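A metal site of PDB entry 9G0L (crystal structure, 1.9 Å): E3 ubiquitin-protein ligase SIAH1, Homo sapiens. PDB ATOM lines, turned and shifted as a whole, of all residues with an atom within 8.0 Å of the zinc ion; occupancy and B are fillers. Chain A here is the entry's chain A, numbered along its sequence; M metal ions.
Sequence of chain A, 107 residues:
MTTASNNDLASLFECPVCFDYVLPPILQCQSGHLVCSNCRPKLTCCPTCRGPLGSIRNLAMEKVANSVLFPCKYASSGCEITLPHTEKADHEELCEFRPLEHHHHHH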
ATOM      1  N   PRO A  71     -22.708 -29.466   0.196  1.00  0.00           N
ATOM      2  CA  PRO A  71     -21.429 -29.106   0.800  1.00  0.00           C
ATOM      3  C   PRO A  71     -21.605 -28.163   1.980  1.00  0.00           C
ATOM      4  O   PRO A  71     -22.486 -27.304   1.988  1.00  0.00           O
ATOM      5  CB  PRO A  71     -20.653 -28.435  -0.334  1.00  0.00           C
ATOM      6  CG  PRO A  71     -21.435 -28.633  -1.567  1.00  0.00           C
ATOM      7  CD  PRO A  71     -22.760 -29.207  -1.250  1.00  0.00           C
ATOM      8  N   CYS A  72     -20.752 -28.346   3.010  1.00  0.00           N
ATOM      9  CA  CYS A  72     -20.696 -27.407   4.117  1.00  0.00           C
ATOM     10  C   CYS A  72     -20.557 -25.982   3.600  1.00  0.00           C
ATOM     11  O   CYS A  72     -19.855 -25.735   2.609  1.00  0.00           O
ATOM     12  CB  CYS A  72     -19.505 -27.744   5.022  1.00  0.00           C
ATOM     13  SG  CYS A  72     -19.260 -26.544   6.351  1.00  0.00           S
ATOM     14  N   LYS A  73     -21.217 -25.031   4.262  1.00  0.00           N
ATOM     15  CA  LYS A  73     -21.088 -23.631   3.849  1.00  0.00           C
ATOM     16  C   LYS A  73     -19.644 -23.162   3.996  1.00  0.00           C
ATOM     17  O   LYS A  73     -19.302 -22.134   3.433  1.00  0.00           O
ATOM     18  CB  LYS A  73     -21.980 -22.713   4.688  1.00  0.00           C
ATOM     19  CG  LYS A  73     -21.445 -22.530   6.093  1.00  0.00           C
ATOM     20  CD  LYS A  73     -22.482 -22.141   7.135  1.00  0.00           C
ATOM     21  CE  LYS A  73     -22.985 -20.754   7.062  1.00  0.00           C
ATOM     22  NZ  LYS A  73     -23.499 -20.435   8.433  1.00  0.00           N
ATOM     23  N   TYR A  74     -18.799 -23.874   4.742  1.00  0.00           N
ATOM     24  CA  TYR A  74     -17.408 -23.468   4.875  1.00  0.00           C
ATOM     25  C   TYR A  74     -16.493 -24.237   3.939  1.00  0.00           C
ATOM     26  O   TYR A  74     -15.301 -24.393   4.217  1.00  0.00           O
ATOM     27  CB  TYR A  74     -16.932 -23.610   6.322  1.00  0.00           C
ATOM     28  CG  TYR A  74     -17.755 -22.819   7.300  1.00  0.00           C
ATOM     29  CD1 TYR A  74     -17.782 -21.435   7.256  1.00  0.00           C
ATOM     30  CD2 TYR A  74     -18.503 -23.463   8.273  1.00  0.00           C
ATOM     31  CE1 TYR A  74     -18.552 -20.707   8.150  1.00  0.00           C
ATOM     32  CE2 TYR A  74     -19.269 -22.742   9.173  1.00  0.00           C
ATOM     33  CZ  TYR A  74     -19.292 -21.362   9.106  1.00  0.00           C
ATOM     34  OH  TYR A  74     -20.049 -20.652  10.006  1.00  0.00           O
ATOM     35  N   ALA A  75     -17.031 -24.728   2.823  1.00  0.00           N
ATOM     36  CA  ALA A  75     -16.181 -25.380   1.830  1.00  0.00           C
ATOM     37  C   ALA A  75     -15.087 -24.439   1.332  1.00  0.00           C
ATOM     38  O   ALA A  75     -13.951 -24.870   1.127  1.00  0.00           O
ATOM     39  CB  ALA A  75     -17.047 -25.878   0.663  1.00  0.00           C
ATOM     40  N   GLY A  78     -12.166 -24.563   3.233  1.00  0.00           N
ATOM     41  CA  GLY A  78     -11.476 -25.836   3.198  1.00  0.00           C
ATOM     42  C   GLY A  78     -12.219 -27.011   3.796  1.00  0.00           C
ATOM     43  O   GLY A  78     -11.625 -28.088   3.924  1.00  0.00           O
ATOM     44  N   CYS A  79     -13.492 -26.868   4.157  1.00  0.00           N
ATOM     45  CA  CYS A  79     -14.260 -28.021   4.615  1.00  0.00           C
ATOM     46  C   CYS A  79     -14.684 -28.855   3.414  1.00  0.00           C
ATOM     47  O   CYS A  79     -15.261 -28.346   2.460  1.00  0.00           O
ATOM     48  CB  CYS A  79     -15.499 -27.592   5.402  1.00  0.00           C
ATOM     49  SG  CYS A  79     -16.359 -29.028   6.032  1.00  0.00           S
ATOM     50  N   GLU A  80     -14.411 -30.152   3.467  1.00  0.00           N
ATOM     51  CA  GLU A  80     -14.767 -31.045   2.375  1.00  0.00           C
ATOM     52  C   GLU A  80     -15.956 -31.922   2.705  1.00  0.00           C
ATOM     53  O   GLU A  80     -16.287 -32.835   1.946  1.00  0.00           O
ATOM     54  CB  GLU A  80     -13.567 -31.904   1.979  1.00  0.00           C
ATOM     55  CG  GLU A  80     -12.251 -31.158   2.044  1.00  0.00           C
ATOM     56  CD  GLU A  80     -11.075 -32.023   1.671  1.00  0.00           C
ATOM     57  OE1 GLU A  80     -11.229 -32.902   0.797  1.00  0.00           O
ATOM     58  OE2 GLU A  80     -10.009 -31.871   2.304  1.00  0.00           O
ATOM     59  N   ILE A  81     -16.621 -31.673   3.814  1.00  0.00           N
ATOM     60  CA  ILE A  81     -17.752 -32.487   4.221  1.00  0.00           C
ATOM     61  C   ILE A  81     -18.977 -32.085   3.390  1.00  0.00           C
ATOM     62  O   ILE A  81     -19.196 -30.906   3.142  1.00  0.00           O
ATOM     63  CB  ILE A  81     -18.017 -32.304   5.727  1.00  0.00           C
ATOM     64  CG1 ILE A  81     -16.782 -32.755   6.544  1.00  0.00           C
ATOM     65  CG2 ILE A  81     -19.279 -33.039   6.146  1.00  0.00           C
ATOM     66  CD1 ILE A  81     -16.175 -34.081   6.087  1.00  0.00           C
ATOM     67  N   THR A  82     -19.734 -33.071   2.909  1.00  0.00           N
ATOM     68  CA  THR A  82     -21.025 -32.827   2.284  1.00  0.00           C
ATOM     69  C   THR A  82     -22.079 -33.601   3.069  1.00  0.00           C
ATOM     70  O   THR A  82     -21.804 -34.706   3.552  1.00  0.00           O
ATOM     71  CB  THR A  82     -21.036 -33.240   0.797  1.00  0.00           C
ATOM     72  OG1 THR A  82     -20.724 -34.631   0.690  1.00  0.00           O
ATOM     73  CG2 THR A  82     -19.990 -32.496   0.047  1.00  0.00           C
ATOM     74  N   LEU A  83     -23.253 -33.006   3.226  1.00  0.00           N
ATOM     75  CA  LEU A  83     -24.175 -33.416   4.282  1.00  0.00           C
ATOM     76  C   LEU A  83     -25.605 -33.502   3.783  1.00  0.00           C
ATOM     77  O   LEU A  83     -26.041 -32.675   2.963  1.00  0.00           O
ATOM     78  CB  LEU A  83     -24.134 -32.414   5.437  1.00  0.00           C
ATOM     79  CG  LEU A  83     -22.801 -32.286   6.148  1.00  0.00           C
ATOM     80  CD1 LEU A  83     -22.482 -30.811   6.243  1.00  0.00           C
ATOM     81  CD2 LEU A  83     -22.957 -32.863   7.494  1.00  0.00           C
ATOM     82  N   LYS A  88     -26.973 -30.417   7.933  1.00  0.00           N
ATOM     83  CA  LYS A  88     -26.052 -29.381   7.487  1.00  0.00           C
ATOM     84  C   LYS A  88     -25.865 -28.317   8.558  1.00  0.00           C
ATOM     85  O   LYS A  88     -24.737 -27.946   8.897  1.00  0.00           O
ATOM     86  CB  LYS A  88     -26.563 -28.767   6.169  1.00  0.00           C
ATOM     87  CG  LYS A  88     -25.578 -27.874   5.429  1.00  0.00           C
ATOM     88  CD  LYS A  88     -25.921 -27.876   3.924  1.00  0.00           C
ATOM     89  CE  LYS A  88     -25.335 -26.701   3.134  1.00  0.00           C
ATOM     90  NZ  LYS A  88     -25.125 -25.457   3.886  1.00  0.00           N
ATOM     91  N   HIS A  91     -23.836 -29.413  11.641  1.00  0.00           N
ATOM     92  CA  HIS A  91     -22.426 -29.559  11.288  1.00  0.00           C
ATOM     93  C   HIS A  91     -21.739 -28.205  11.231  1.00  0.00           C
ATOM     94  O   HIS A  91     -20.659 -28.015  11.805  1.00  0.00           O
ATOM     95  CB  HIS A  91     -22.255 -30.267   9.947  1.00  0.00           C
ATOM     96  CG  HIS A  91     -20.902 -30.076   9.352  1.00  0.00           C
ATOM     97  ND1 HIS A  91     -19.811 -30.841   9.716  1.00  0.00           N
ATOM     98  CD2 HIS A  91     -20.435 -29.176   8.447  1.00  0.00           C
ATOM     99  CE1 HIS A  91     -18.746 -30.435   9.049  1.00  0.00           C
ATOM    100  NE2 HIS A  91     -19.104 -29.430   8.267  1.00  0.00           N
ATOM    101  N   GLU A  92     -22.350 -27.249  10.537  1.00  0.00           N
ATOM    102  CA  GLU A  92     -21.727 -25.954  10.333  1.00  0.00           C
ATOM    103  C   GLU A  92     -21.541 -25.214  11.642  1.00  0.00           C
ATOM    104  O   GLU A  92     -20.634 -24.382  11.757  1.00  0.00           O
ATOM    105  CB  GLU A  92     -22.564 -25.143   9.345  1.00  0.00           C
ATOM    106  CG  GLU A  92     -22.579 -25.754   7.952  1.00  0.00           C
ATOM    107  CD  GLU A  92     -23.610 -25.161   7.003  1.00  0.00           C
ATOM    108  OE1 GLU A  92     -24.538 -24.451   7.442  1.00  0.00           O
ATOM    109  OE2 GLU A  92     -23.465 -25.408   5.789  1.00  0.00           O
ATOM    110  N   GLU A  93     -22.354 -25.533  12.652  1.00  0.00           N
ATOM    111  CA  GLU A  93     -22.219 -24.845  13.928  1.00  0.00           C
ATOM    112  C   GLU A  93     -20.952 -25.279  14.668  1.00  0.00           C
ATOM    113  O   GLU A  93     -20.390 -24.495  15.434  1.00  0.00           O
ATOM    114  CB  GLU A  93     -23.516 -25.079  14.719  1.00  0.00           C
ATOM    115  CG  GLU A  93     -23.415 -25.210  16.208  1.00  0.00           C
ATOM    116  CD  GLU A  93     -24.795 -25.141  16.877  1.00  0.00           C
ATOM    117  OE1 GLU A  93     -25.815 -25.415  16.191  1.00  0.00           O
ATOM    118  OE2 GLU A  93     -24.863 -24.805  18.074  1.00  0.00           O
ATOM    119  N   LEU A  94     -20.455 -26.495  14.410  1.00  0.00           N
ATOM    120  CA  LEU A  94     -19.237 -26.984  15.046  1.00  0.00           C
ATOM    121  C   LEU A  94     -18.089 -27.193  14.060  1.00  0.00           C
ATOM    122  O   LEU A  94     -17.030 -27.710  14.454  1.00  0.00           O
ATOM    123  CB  LEU A  94     -19.557 -28.292  15.791  1.00  0.00           C
ATOM    124  CG  LEU A  94     -20.567 -28.151  16.934  1.00  0.00           C
ATOM    125  CD1 LEU A  94     -21.068 -29.508  17.408  1.00  0.00           C
ATOM    126  CD2 LEU A  94     -20.019 -27.331  18.104  1.00  0.00           C
ATOM    127  N   CYS A  95     -18.262 -26.794  12.805  1.00  0.00           N
ATOM    128  CA  CYS A  95     -17.305 -27.133  11.765  1.00  0.00           C
ATOM    129  C   CYS A  95     -15.913 -26.604  12.072  1.00  0.00           C
ATOM    130  O   CYS A  95     -15.741 -25.452  12.464  1.00  0.00           O
ATOM    131  CB  CYS A  95     -17.756 -26.598  10.422  1.00  0.00           C
ATOM    132  SG  CYS A  95     -16.616 -26.981   9.110  1.00  0.00           S
ATOM    133  N   GLU A  96     -14.906 -27.477  11.857  1.00  0.00           N
ATOM    134  CA  GLU A  96     -13.498 -27.106  12.021  1.00  0.00           C
ATOM    135  C   GLU A  96     -13.163 -25.786  11.331  1.00  0.00           C
ATOM    136  O   GLU A  96     -12.346 -25.003  11.838  1.00  0.00           O
ATOM    137  CB  GLU A  96     -12.601 -28.214  11.444  1.00  0.00           C
ATOM    138  CG  GLU A  96     -11.119 -27.871  11.458  1.00  0.00           C
ATOM    139  CD  GLU A  96     -10.213 -29.028  11.045  1.00  0.00           C
ATOM    140  OE1 GLU A  96      -8.988 -28.817  10.892  1.00  0.00           O
ATOM    141  OE2 GLU A  96     -10.735 -30.139  10.799  1.00  0.00           O
ATOM    142  N   PHE A  97     -13.773 -25.522  10.175  1.00  0.00           N
ATOM    143  CA  PHE A  97     -13.385 -24.393   9.334  1.00  0.00           C
ATOM    144  C   PHE A  97     -14.272 -23.175   9.501  1.00  0.00           C
ATOM    145  O   PHE A  97     -14.234 -22.279   8.650  1.00  0.00           O
ATOM    146  CB  PHE A  97     -13.344 -24.845   7.872  1.00  0.00           C
ATOM    147  CG  PHE A  97     -12.438 -25.999   7.623  1.00  0.00           C
ATOM    148  CD1 PHE A  97     -11.098 -25.786   7.334  1.00  0.00           C
ATOM    149  CD2 PHE A  97     -12.900 -27.298   7.725  1.00  0.00           C
ATOM    150  CE1 PHE A  97     -10.240 -26.861   7.137  1.00  0.00           C
ATOM    151  CE2 PHE A  97     -12.055 -28.365   7.511  1.00  0.00           C
ATOM    152  CZ  PHE A  97     -10.725 -28.142   7.222  1.00  0.00           C
ATOM    153  N   ARG A  98     -15.082 -23.111  10.567  1.00  0.00           N
ATOM    154  CA  ARG A  98     -15.806 -21.859  10.740  1.00  0.00           C
ATOM    155  C   ARG A  98     -14.868 -20.783  11.282  1.00  0.00           C
ATOM    156  O   ARG A  98     -13.868 -21.091  11.932  1.00  0.00           O
ATOM    157  CB  ARG A  98     -16.991 -22.037  11.683  1.00  0.00           C
ATOM    158  CG  ARG A  98     -16.657 -22.073  13.164  1.00  0.00           C
ATOM    159  CD  ARG A  98     -17.430 -23.191  13.843  1.00  0.00           C
ATOM    160  NE  ARG A  98     -17.346 -23.146  15.301  1.00  0.00           N
ATOM    161  CZ  ARG A  98     -16.417 -23.751  16.015  1.00  0.00           C
ATOM    162  NH1 ARG A  98     -15.471 -24.487  15.441  1.00  0.00           N
ATOM    163  NH2 ARG A  98     -16.435 -23.643  17.342  1.00  0.00           N
HETATM  164 ZN    ZN M   1     -17.821 -28.001   7.463  1.00  0.00          ZN
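SG of Cys 95 lies close to N of Phe 97 (3.4 Å). The backbone carbonyl oxygen of Cys 95 lies close to the guanidinium group of Arg 98 (3.1 Å). N of Cys 79 lies within hydrogen-bond range of O of Tyr 74 (3.1 Å). The side-chain sulfur (SG) of Cys 79 lies close to the backbone NH (N) of Ile 81. The side-chain sulfur of Cys 72 lies close to the backbone NH of Tyr 74 (3.2 Å). The backbone NH (N) of Cys 72 is in hydrogen-bond range of the backbone carbonyl oxygen (O) of Ile 81 (3.0 Å).
The nearest printed residue that does not touch the zinc ion is Tyr 74 (4.6 Å).
The zinc ion is bound by NE2 of His 91 (2.1 Å). The side-chain sulfur (SG) of Cys 95 binds the zinc ion. SG of Cys 79 binds the zinc ion (2.3 Å). The zinc ion is bound by the side-chain sulfur (SG) of Cys 72. The zinc ion has four donor atoms within binding distance.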
